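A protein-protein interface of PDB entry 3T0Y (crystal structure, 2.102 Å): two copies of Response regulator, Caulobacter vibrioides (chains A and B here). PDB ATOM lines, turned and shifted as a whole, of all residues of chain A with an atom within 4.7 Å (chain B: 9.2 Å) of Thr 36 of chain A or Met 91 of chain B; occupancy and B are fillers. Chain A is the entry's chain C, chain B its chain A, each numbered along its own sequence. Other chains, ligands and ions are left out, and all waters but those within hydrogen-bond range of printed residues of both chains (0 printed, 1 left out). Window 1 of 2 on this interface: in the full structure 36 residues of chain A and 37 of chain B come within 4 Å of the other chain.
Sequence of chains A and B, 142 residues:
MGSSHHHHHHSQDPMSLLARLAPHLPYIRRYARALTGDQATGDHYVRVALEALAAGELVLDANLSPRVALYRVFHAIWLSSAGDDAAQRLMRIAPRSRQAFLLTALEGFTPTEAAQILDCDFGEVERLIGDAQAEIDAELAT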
ATOM      1  N   ALA A  32      22.358  10.927   8.704  1.00  0.00           N
ATOM      2  CA  ALA A  32      23.197  10.071   9.523  1.00  0.00           C
ATOM      3  C   ALA A  32      22.638   8.667   9.576  1.00  0.00           C
ATOM      4  O   ALA A  32      23.369   7.686   9.383  1.00  0.00           O
ATOM      5  CB  ALA A  32      23.309  10.666  10.949  1.00  0.00           C
ATOM      6  N   ARG A  33      21.325   8.577   9.805  1.00  0.00           N
ATOM      7  CA  ARG A  33      20.640   7.297   9.949  1.00  0.00           C
ATOM      8  C   ARG A  33      20.632   6.562   8.615  1.00  0.00           C
ATOM      9  O   ARG A  33      20.856   5.359   8.563  1.00  0.00           O
ATOM     10  CB  ARG A  33      19.226   7.503  10.530  1.00  0.00           C
ATOM     11  CG  ARG A  33      18.025   6.835   9.807  1.00  0.00           C
ATOM     12  CD  ARG A  33      18.071   5.315   9.823  1.00  0.00           C
ATOM     13  NE  ARG A  33      16.794   4.585   9.947  1.00  0.00           N
ATOM     14  CZ  ARG A  33      15.556   5.096   9.918  1.00  0.00           C
ATOM     15  NH1 ARG A  33      15.337   6.394   9.737  1.00  0.00           N
ATOM     16  NH2 ARG A  33      14.513   4.280  10.064  1.00  0.00           N
ATOM     17  N   ALA A  34      20.420   7.285   7.525  1.00  0.00           N
ATOM     18  CA  ALA A  34      20.332   6.621   6.237  1.00  0.00           C
ATOM     19  C   ALA A  34      21.712   6.107   5.836  1.00  0.00           C
ATOM     20  O   ALA A  34      21.833   5.051   5.207  1.00  0.00           O
ATOM     21  CB  ALA A  34      19.784   7.580   5.188  1.00  0.00           C
ATOM     22  N   LEU A  35      22.750   6.858   6.202  1.00  0.00           N
ATOM     23  CA  LEU A  35      24.106   6.531   5.779  1.00  0.00           C
ATOM     24  C   LEU A  35      24.663   5.382   6.577  1.00  0.00           C
ATOM     25  O   LEU A  35      25.300   4.500   6.010  1.00  0.00           O
ATOM     26  CB  LEU A  35      25.045   7.742   5.892  1.00  0.00           C
ATOM     27  CG  LEU A  35      26.534   7.497   5.595  1.00  0.00           C
ATOM     28  CD1 LEU A  35      26.793   7.311   4.074  1.00  0.00           C
ATOM     29  CD2 LEU A  35      27.409   8.622   6.141  1.00  0.00           C
ATOM     30  N   THR A  36      24.392   5.359   7.882  1.00  0.00           N
ATOM     31  CA  THR A  36      25.101   4.445   8.766  1.00  0.00           C
ATOM     32  C   THR A  36      24.278   3.256   9.297  1.00  0.00           C
ATOM     33  O   THR A  36      24.827   2.370   9.945  1.00  0.00           O
ATOM     34  CB  THR A  36      25.701   5.191   9.963  1.00  0.00           C
ATOM     35  OG1 THR A  36      24.638   5.576  10.838  1.00  0.00           O
ATOM     36  CG2 THR A  36      26.478   6.436   9.498  1.00  0.00           C
ATOM     37  N   GLY A  37      22.971   3.242   9.036  1.00  0.00           N
ATOM     38  CA  GLY A  37      22.204   2.034   9.237  1.00  0.00           C
ATOM     39  C   GLY A  37      21.066   2.057  10.223  1.00  0.00           C
ATOM     40  O   GLY A  37      20.126   1.270  10.086  1.00  0.00           O
ATOM     41  N   ASP A  38      21.170   2.916  11.230  1.00  0.00           N
ATOM     42  CA  ASP A  38      20.097   3.119  12.194  1.00  0.00           C
ATOM     43  C   ASP A  38      20.312   4.425  12.962  1.00  0.00           C
ATOM     44  O   ASP A  38      21.358   5.079  12.821  1.00  0.00           O
ATOM     45  CB  ASP A  38      19.946   1.916  13.145  1.00  0.00           C
ATOM     46  CG  ASP A  38      21.123   1.756  14.110  1.00  0.00           C
ATOM     47  OD1 ASP A  38      21.146   0.750  14.855  1.00  0.00           O
ATOM     48  OD2 ASP A  38      22.018   2.623  14.141  1.00  0.00           O
ATOM     49  N   THR A  41      23.370   4.544  15.617  1.00  0.00           N
ATOM     50  CA  THR A  41      24.631   4.733  14.932  1.00  0.00           C
ATOM     51  C   THR A  41      24.704   6.168  14.362  1.00  0.00           C
ATOM     52  O   THR A  41      25.734   6.855  14.509  1.00  0.00           O
ATOM     53  CB  THR A  41      24.827   3.685  13.819  1.00  0.00           C
ATOM     54  OG1 THR A  41      24.672   2.364  14.365  1.00  0.00           O
ATOM     55  CG2 THR A  41      26.218   3.801  13.218  1.00  0.00           C
ATOM     56  N   GLY A  42      23.607   6.635  13.761  1.00  0.00           N
ATOM     57  CA  GLY A  42      23.592   7.979  13.173  1.00  0.00           C
ATOM     58  C   GLY A  42      23.787   9.083  14.217  1.00  0.00           C
ATOM     59  O   GLY A  42      24.584  10.009  14.034  1.00  0.00           O
ATOM     60  N   TYR A  45      27.312   9.548  15.383  1.00  0.00           N
ATOM     61  CA  TYR A  45      28.191  10.295  14.487  1.00  0.00           C
ATOM     62  C   TYR A  45      27.889  11.794  14.502  1.00  0.00           C
ATOM     63  O   TYR A  45      28.787  12.631  14.384  1.00  0.00           O
ATOM     64  CB  TYR A  45      28.110   9.730  13.062  1.00  0.00           C
ATOM     65  CG  TYR A  45      29.012   8.541  12.857  1.00  0.00           C
ATOM     66  CD1 TYR A  45      30.399   8.695  12.884  1.00  0.00           C
ATOM     67  CD2 TYR A  45      28.490   7.266  12.666  1.00  0.00           C
ATOM     68  CE1 TYR A  45      31.243   7.613  12.707  1.00  0.00           C
ATOM     69  CE2 TYR A  45      29.330   6.165  12.482  1.00  0.00           C
ATOM     70  CZ  TYR A  45      30.707   6.355  12.503  1.00  0.00           C
ATOM     71  OH  TYR A  45      31.555   5.297  12.311  1.00  0.00           O
ATOM     72  N   TRP A  78      33.006  11.318  10.097  1.00  0.00           N
ATOM     73  CA  TRP A  78      32.516   9.998   9.717  1.00  0.00           C
ATOM     74  C   TRP A  78      33.609   9.228   8.997  1.00  0.00           C
ATOM     75  O   TRP A  78      33.901   8.071   9.306  1.00  0.00           O
ATOM     76  CB  TRP A  78      31.298  10.108   8.803  1.00  0.00           C
ATOM     77  CG  TRP A  78      30.873   8.785   8.289  1.00  0.00           C
ATOM     78  CD1 TRP A  78      30.204   7.817   8.975  1.00  0.00           C
ATOM     79  CD2 TRP A  78      31.089   8.270   6.974  1.00  0.00           C
ATOM     80  NE1 TRP A  78      29.998   6.718   8.170  1.00  0.00           N
ATOM     81  CE2 TRP A  78      30.522   6.976   6.931  1.00  0.00           C
ATOM     82  CE3 TRP A  78      31.709   8.774   5.827  1.00  0.00           C
ATOM     83  CZ2 TRP A  78      30.567   6.174   5.788  1.00  0.00           C
ATOM     84  CZ3 TRP A  78      31.740   7.987   4.692  1.00  0.00           C
ATOM     85  CH2 TRP A  78      31.168   6.695   4.681  1.00  0.00           C
ATOM     86  N   ALA A  94      27.650  -2.042   9.703  1.00  0.00           N
ATOM     87  CA  ALA A  94      26.189  -2.066   9.710  1.00  0.00           C
ATOM     88  C   ALA A  94      25.743  -2.645  11.029  1.00  0.00           C
ATOM     89  O   ALA A  94      26.265  -3.676  11.457  1.00  0.00           O
ATOM     90  CB  ALA A  94      25.645  -2.907   8.563  1.00  0.00           C
ATOM     91  N   PRO A  95      24.782  -1.983  11.681  1.00  0.00           N
ATOM     92  CA  PRO A  95      24.299  -2.363  13.016  1.00  0.00           C
ATOM     93  C   PRO A  95      23.996  -3.863  13.196  1.00  0.00           C
ATOM     94  O   PRO A  95      24.440  -4.442  14.190  1.00  0.00           O
ATOM     95  CB  PRO A  95      23.034  -1.517  13.180  1.00  0.00           C
ATOM     96  CG  PRO A  95      23.339  -0.259  12.368  1.00  0.00           C
ATOM     97  CD  PRO A  95      24.140  -0.755  11.186  1.00  0.00           C
ATOM     98  N   GLY B  83      13.323   0.972   7.697  1.00  0.00           N
ATOM     99  CA  GLY B  83      14.260   1.956   7.189  1.00  0.00           C
ATOM    100  C   GLY B  83      15.688   1.527   7.484  1.00  0.00           C
ATOM    101  O   GLY B  83      16.602   1.752   6.687  1.00  0.00           O
ATOM    102  N   ASP B  84      15.870   0.901   8.641  1.00  0.00           N
ATOM    103  CA  ASP B  84      17.180   0.435   9.064  1.00  0.00           C
ATOM    104  C   ASP B  84      17.673  -0.645   8.096  1.00  0.00           C
ATOM    105  O   ASP B  84      18.858  -0.685   7.735  1.00  0.00           O
ATOM    106  CB  ASP B  84      17.115  -0.125  10.489  1.00  0.00           C
ATOM    107  CG  ASP B  84      16.812   0.947  11.541  1.00  0.00           C
ATOM    108  OD1 ASP B  84      16.465   0.574  12.691  1.00  0.00           O
ATOM    109  OD2 ASP B  84      16.928   2.154  11.234  1.00  0.00           O
ATOM    110  N   ASP B  85      16.755  -1.507   7.666  1.00  0.00           N
ATOM    111  CA  ASP B  85      17.100  -2.598   6.758  1.00  0.00           C
ATOM    112  C   ASP B  85      17.414  -2.052   5.361  1.00  0.00           C
ATOM    113  O   ASP B  85      18.352  -2.501   4.706  1.00  0.00           O
ATOM    114  CB  ASP B  85      15.973  -3.642   6.692  1.00  0.00           C
ATOM    115  CG  ASP B  85      15.645  -4.266   8.068  1.00  0.00           C
ATOM    116  OD1 ASP B  85      16.580  -4.601   8.848  1.00  0.00           O
ATOM    117  OD2 ASP B  85      14.434  -4.421   8.360  1.00  0.00           O
ATOM    118  N   ALA B  86      16.636  -1.075   4.909  1.00  0.00           N
ATOM    119  CA  ALA B  86      16.937  -0.433   3.632  1.00  0.00           C
ATOM    120  C   ALA B  86      18.324   0.230   3.691  1.00  0.00           C
ATOM    121  O   ALA B  86      19.168   0.001   2.831  1.00  0.00           O
ATOM    122  CB  ALA B  86      15.854   0.569   3.265  1.00  0.00           C
ATOM    123  N   ALA B  87      18.565   1.014   4.733  1.00  0.00           N
ATOM    124  CA  ALA B  87      19.861   1.665   4.925  1.00  0.00           C
ATOM    125  C   ALA B  87      21.011   0.661   4.936  1.00  0.00           C
ATOM    126  O   ALA B  87      22.109   0.933   4.419  1.00  0.00           O
ATOM    127  CB  ALA B  87      19.860   2.472   6.209  1.00  0.00           C
ATOM    128  N   GLN B  88      20.759  -0.504   5.519  1.00  0.00           N
ATOM    129  CA  GLN B  88      21.805  -1.517   5.633  1.00  0.00           C
ATOM    130  C   GLN B  88      22.038  -2.277   4.325  1.00  0.00           C
ATOM    131  O   GLN B  88      23.180  -2.566   3.963  1.00  0.00           O
ATOM    132  CB  GLN B  88      21.555  -2.417   6.845  1.00  0.00           C
ATOM    133  CG  GLN B  88      21.815  -1.639   8.133  1.00  0.00           C
ATOM    134  CD  GLN B  88      21.489  -2.408   9.382  1.00  0.00           C
ATOM    135  OE1 GLN B  88      22.193  -3.355   9.747  1.00  0.00           O
ATOM    136  NE2 GLN B  88      20.427  -1.991  10.067  1.00  0.00           N
ATOM    137  N   ARG B  89      20.955  -2.545   3.605  1.00  0.00           N
ATOM    138  CA  ARG B  89      21.025  -2.999   2.220  1.00  0.00           C
ATOM    139  C   ARG B  89      21.929  -2.056   1.400  1.00  0.00           C
ATOM    140  O   ARG B  89      22.904  -2.489   0.759  1.00  0.00           O
ATOM    141  CB  ARG B  89      19.610  -3.025   1.624  1.00  0.00           C
ATOM    142  CG  ARG B  89      19.147  -4.381   1.102  1.00  0.00           C
ATOM    143  CD  ARG B  89      17.680  -4.351   0.612  1.00  0.00           C
ATOM    144  NE  ARG B  89      16.693  -4.217   1.695  1.00  0.00           N
ATOM    145  CZ  ARG B  89      15.635  -3.401   1.661  1.00  0.00           C
ATOM    146  NH1 ARG B  89      15.415  -2.626   0.601  1.00  0.00           N
ATOM    147  NH2 ARG B  89      14.797  -3.352   2.692  1.00  0.00           N
ATOM    148  N   LEU B  90      21.612  -0.759   1.436  1.00  0.00           N
ATOM    149  CA  LEU B  90      22.371   0.223   0.664  1.00  0.00           C
ATOM    150  C   LEU B  90      23.859   0.233   1.053  1.00  0.00           C
ATOM    151  O   LEU B  90      24.728   0.365   0.201  1.00  0.00           O
ATOM    152  CB  LEU B  90      21.760   1.610   0.821  1.00  0.00           C
ATOM    153  CG  LEU B  90      22.418   2.697  -0.016  1.00  0.00           C
ATOM    154  CD1 LEU B  90      22.187   2.427  -1.506  1.00  0.00           C
ATOM    155  CD2 LEU B  90      21.880   4.079   0.388  1.00  0.00           C
ATOM    156  N   MET B  91      24.141   0.076   2.339  1.00  0.00           N
ATOM    157  CA  MET B  91      25.515   0.004   2.830  1.00  0.00           C
ATOM    158  C   MET B  91      26.274  -1.144   2.176  1.00  0.00           C
ATOM    159  O   MET B  91      27.499  -1.092   2.030  1.00  0.00           O
ATOM    160  CB  MET B  91      25.511  -0.220   4.342  1.00  0.00           C
ATOM    161  CG  MET B  91      25.835   0.995   5.185  1.00  0.00           C
ATOM    162  SD  MET B  91      25.534   0.630   7.076  1.00  0.00           S
ATOM    163  CE  MET B  91      23.625   0.873   6.944  1.00  0.00           C
ATOM    164  N   ARG B  92      25.538  -2.194   1.812  1.00  0.00           N
ATOM    165  CA  ARG B  92      26.121  -3.385   1.192  1.00  0.00           C
ATOM    166  C   ARG B  92      26.249  -3.211  -0.332  1.00  0.00           C
ATOM    167  O   ARG B  92      27.265  -3.557  -0.943  1.00  0.00           O
ATOM    168  CB  ARG B  92      25.249  -4.604   1.531  1.00  0.00           C
ATOM    169  CG  ARG B  92      26.012  -5.864   1.909  1.00  0.00           C
ATOM    170  CD  ARG B  92      25.070  -6.929   2.498  1.00  0.00           C
ATOM    171  NE  ARG B  92      24.447  -6.491   3.752  1.00  0.00           N
ATOM    172  CZ  ARG B  92      23.131  -6.355   3.945  1.00  0.00           C
ATOM    173  NH1 ARG B  92      22.272  -6.629   2.964  1.00  0.00           N
ATOM    174  NH2 ARG B  92      22.668  -5.948   5.126  1.00  0.00           N
ATOM    175  N   ILE B  93      25.206  -2.647  -0.930  1.00  0.00           N
ATOM    176  CA  ILE B  93      25.130  -2.418  -2.371  1.00  0.00           C
ATOM    177  C   ILE B  93      26.085  -1.323  -2.844  1.00  0.00           C
ATOM    178  O   ILE B  93      26.673  -1.431  -3.916  1.00  0.00           O
ATOM    179  CB  ILE B  93      23.700  -1.969  -2.762  1.00  0.00           C
ATOM    180  CG1 ILE B  93      22.734  -3.150  -2.687  1.00  0.00           C
ATOM    181  CG2 ILE B  93      23.677  -1.397  -4.138  1.00  0.00           C
ATOM    182  CD1 ILE B  93      21.327  -2.768  -3.061  1.00  0.00           C
ATOM    183  N   ALA B  94      26.223  -0.262  -2.049  1.00  0.00           N
ATOM    184  CA  ALA B  94      26.982   0.928  -2.454  1.00  0.00           C
ATOM    185  C   ALA B  94      27.949   1.403  -1.352  1.00  0.00           C
ATOM    186  O   ALA B  94      27.827   2.518  -0.846  1.00  0.00           O
ATOM    187  CB  ALA B  94      26.017   2.052  -2.859  1.00  0.00           C
ATOM    188  N   PRO B  95      28.930   0.558  -0.997  1.00  0.00           N
ATOM    189  CA  PRO B  95      29.773   0.788   0.184  1.00  0.00           C
ATOM    190  C   PRO B  95      30.667   2.033   0.129  1.00  0.00           C
ATOM    191  O   PRO B  95      30.993   2.581   1.177  1.00  0.00           O
ATOM    192  CB  PRO B  95      30.615  -0.500   0.277  1.00  0.00           C
ATOM    193  CG  PRO B  95      30.592  -1.068  -1.114  1.00  0.00           C
ATOM    194  CD  PRO B  95      29.250  -0.712  -1.676  1.00  0.00           C
ATOM    195  N   ARG B  96      31.051   2.481  -1.061  1.00  0.00           N
ATOM    196  CA  ARG B  96      31.989   3.597  -1.153  1.00  0.00           C
ATOM    197  C   ARG B  96      31.391   4.842  -1.791  1.00  0.00           C
ATOM    198  O   ARG B  96      32.023   5.905  -1.799  1.00  0.00           O
ATOM    199  CB  ARG B  96      33.250   3.180  -1.920  1.00  0.00           C
ATOM    200  CG  ARG B  96      34.172   2.228  -1.153  1.00  0.00           C
ATOM    201  CD  ARG B  96      35.136   1.485  -2.081  1.00  0.00           C
ATOM    202  NE  ARG B  96      36.248   2.315  -2.548  1.00  0.00           N
ATOM    203  CZ  ARG B  96      37.202   1.893  -3.377  1.00  0.00           C
ATOM    204  NH1 ARG B  96      37.181   0.645  -3.840  1.00  0.00           N
ATOM    205  NH2 ARG B  96      38.181   2.715  -3.748  1.00  0.00           N
ATOM    206  N   SER B  97      30.171   4.734  -2.303  1.00  0.00           N
ATOM    207  CA  SER B  97      29.613   5.809  -3.128  1.00  0.00           C
ATOM    208  C   SER B  97      28.237   6.277  -2.683  1.00  0.00           C
ATOM    209  O   SER B  97      27.729   7.261  -3.206  1.00  0.00           O
ATOM    210  CB  SER B  97      29.484   5.307  -4.560  1.00  0.00           C
ATOM    211  OG  SER B  97      28.700   4.125  -4.552  1.00  0.00           O
ATOM    212  N   ARG B  98      27.609   5.570  -1.745  1.00  0.00           N
ATOM    213  CA  ARG B  98      26.232   5.889  -1.386  1.00  0.00           C
ATOM    214  C   ARG B  98      26.086   7.265  -0.769  1.00  0.00           C
ATOM    215  O   ARG B  98      24.991   7.831  -0.792  1.00  0.00           O
ATOM    216  CB  ARG B  98      25.619   4.844  -0.452  1.00  0.00           C
ATOM    217  CG  ARG B  98      25.990   4.960   1.001  1.00  0.00           C
ATOM    218  CD  ARG B  98      25.640   3.656   1.730  1.00  0.00           C
ATOM    219  NE  ARG B  98      26.167   3.625   3.092  1.00  0.00           N
ATOM    220  CZ  ARG B  98      27.433   3.361   3.407  1.00  0.00           C
ATOM    221  NH1 ARG B  98      28.320   3.097   2.459  1.00  0.00           N
ATOM    222  NH2 ARG B  98      27.819   3.364   4.675  1.00  0.00           N
ATOM    223  N   GLN B  99      27.165   7.795  -0.198  1.00  0.00           N
ATOM    224  CA  GLN B  99      27.081   9.096   0.450  1.00  0.00           C
ATOM    225  C   GLN B  99      26.690  10.180  -0.566  1.00  0.00           C
ATOM    226  O   GLN B  99      25.893  11.070  -0.268  1.00  0.00           O
ATOM    227  CB  GLN B  99      28.401   9.452   1.166  1.00  0.00           C
ATOM    228  CG  GLN B  99      29.620   9.495   0.266  1.00  0.00           C
ATOM    229  CD  GLN B  99      30.358   8.159   0.215  1.00  0.00           C
ATOM    230  OE1 GLN B  99      29.791   7.107   0.508  1.00  0.00           O
ATOM    231  NE2 GLN B  99      31.629   8.204  -0.160  1.00  0.00           N
ATOM    232  N   LEU B 102      23.172   9.864  -1.523  1.00  0.00           N
ATOM    233  CA  LEU B 102      22.266  10.281  -0.454  1.00  0.00           C
ATOM    234  C   LEU B 102      22.224  11.798  -0.305  1.00  0.00           C
ATOM    235  O   LEU B 102      21.150  12.390  -0.148  1.00  0.00           O
ATOM    236  CB  LEU B 102      22.645   9.638   0.873  1.00  0.00           C
ATOM    237  CG  LEU B 102      22.410   8.133   1.031  1.00  0.00           C
ATOM    238  CD1 LEU B 102      23.078   7.700   2.340  1.00  0.00           C
ATOM    239  CD2 LEU B 102      20.918   7.750   1.017  1.00  0.00           C
ATOM    240  N   GLU B 135      24.871   0.546  -9.118  1.00  0.00           N
ATOM    241  CA  GLU B 135      24.755  -0.551  -8.171  1.00  0.00           C
ATOM    242  C   GLU B 135      23.315  -0.754  -7.732  1.00  0.00           C
ATOM    243  O   GLU B 135      22.847  -1.878  -7.596  1.00  0.00           O
ATOM    244  CB  GLU B 135      25.700  -0.320  -6.986  1.00  0.00           C
ATOM    245  CG  GLU B 135      27.149  -0.232  -7.469  1.00  0.00           C
ATOM    246  CD  GLU B 135      28.155   0.065  -6.359  1.00  0.00           C
ATOM    247  OE1 GLU B 135      28.069   1.153  -5.772  1.00  0.00           O
ATOM    248  OE2 GLU B 135      29.035  -0.787  -6.076  1.00  0.00           O
ATOM    249  N   ILE B 136      22.611   0.341  -7.513  1.00  0.00           N
ATOM    250  CA  ILE B 136      21.196   0.268  -7.182  1.00  0.00           C
ATOM    251  C   ILE B 136      20.386  -0.329  -8.344  1.00  0.00           C
ATOM    252  O   ILE B 136      19.648  -1.288  -8.154  1.00  0.00           O
ATOM    253  CB  ILE B 136      20.632   1.658  -6.832  1.00  0.00           C
ATOM    254  CG1 ILE B 136      21.271   2.192  -5.543  1.00  0.00           C
ATOM    255  CG2 ILE B 136      19.111   1.604  -6.702  1.00  0.00           C
ATOM    256  CD1 ILE B 136      20.847   3.583  -5.221  1.00  0.00           C
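Positions printed for both chains: 94 and 95.
The side-chain carboxylate (OD2) of Asp 84 of chain B lies within salt-bridge range of the guanidinium group (NE) of Arg 33 of chain A, 2.8 Å away.
The backbone carbonyl oxygen of Gly 37 of chain A sits at hydrogen-bond distance from the side-chain amide nitrogen of Gln 88 of chain B.
The backbone carbonyl oxygen (O) of Leu 35 of chain A sits at hydrogen-bond distance from the guanidinium group (NH2) of Arg 98 of chain B (3.1 Å).
O of Thr 36 of chain A lies close to SD of Met 91 of chain B, at 3.4 Å.
The backbone carbonyl oxygen of Gly 37 of chain A sits close to the backbone carbonyl oxygen of Asp 84 of chain B, at 3.3 Å.
NE2 of Gln 88 of chain B lies within hydrogen-bond range of O of Asp 84 of chain B (3.1 Å).
The guanidinium group of Arg 98 of chain B sits close to the backbone carbonyl oxygen of Ala 94 of chain B, at 3.4 Å.
NH1 of Arg 98 of chain B sits at hydrogen-bond distance from O of Pro 95 of chain B.
O of Arg 96 of chain B sits at hydrogen-bond distance from NE2 of Gln 99 of chain B (2.9 Å).
The backbone carbonyl oxygen (O) of Ala 32 of chain A lies within hydrogen-bond range of the side-chain hydroxyl (OG1) of Thr 36 of chain A, 2.9 Å away.
The backbone NH of Gly 42 of chain A lies within hydrogen-bond range of the side-chain hydroxyl of Thr 36 of chain A.
Of the 13 printed residues of chain A, 8 touch a printed residue of chain B.
Printed residues of chain A that touch a printed residue of chain B: Arg 33, Ala 34, Leu 35, Thr 36, Gly 37, Asp 38, Ala 94 and Pro 95.
Among the printed residues, merely in contact across the chains: Arg 33 of chain A with Gly 83 of chain B (3.7 Å), Arg 33 of chain A with Ala 87 of chain B (3.9 Å), Ala 34 of chain A with Ala 87 of chain B (3.4 Å), Leu 35 of chain A with Met 91 of chain B (3.6 Å), Leu 35 of chain A with Gln 99 of chain B (3.95 Å), Leu 35 of chain A with Leu 102 of chain B (3.8 Å), Gly 37 of chain A with Ala 87 of chain B (3.9 Å), Gly 37 of chain A with Met 91 of chain B (2.9 Å), Asp 38 of chain A with Asp 84 of chain B (3.4 Å), Ala 94 of chain A with Gln 88 of chain B (3.7 Å), Ala 94 of chain A with Met 91 of chain B (3.8 Å) and Pro 95 of chain A with Gln 88 of chain B (3.5 Å).
Thr 36 of chain A touches just one residue of chain B: Met 91 (3.4 Å).
Met 91 of chain B touches just these residues of chain A: Leu 35, Thr 36, Gly 37 and Ala 94.
Of chain B, only Met 91 (3.6 Å), Arg 98 (3.1 Å), Gln 99 (3.95 Å) and Leu 102 (3.8 Å) come within 4 Å of Leu 35 of chain A.
Gly 37 of chain A touches four residues of chain B.
No residue of chain B comes within 4 Å of Thr 41 of chain A.
Printed residues of chain A within 4 Å of Gln 99 of chain B: Leu 35 (3.95 Å).
Printed residues of chain A within 4 Å of Asp 84 of chain B: Arg 33, Gly 37 and Asp 38.
Ile 136 of chain B touches none of the printed residues of chain A.
Pro 95 of chain B touches none of the printed residues of chain A.
The nearest residue of chain B that does not touch Thr 36 of chain A is Arg 98 of chain B (5.0 Å).
The nearest printed residue of chain A that does not touch Leu 102 of chain B is Ala 34 of chain A (4.1 Å).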
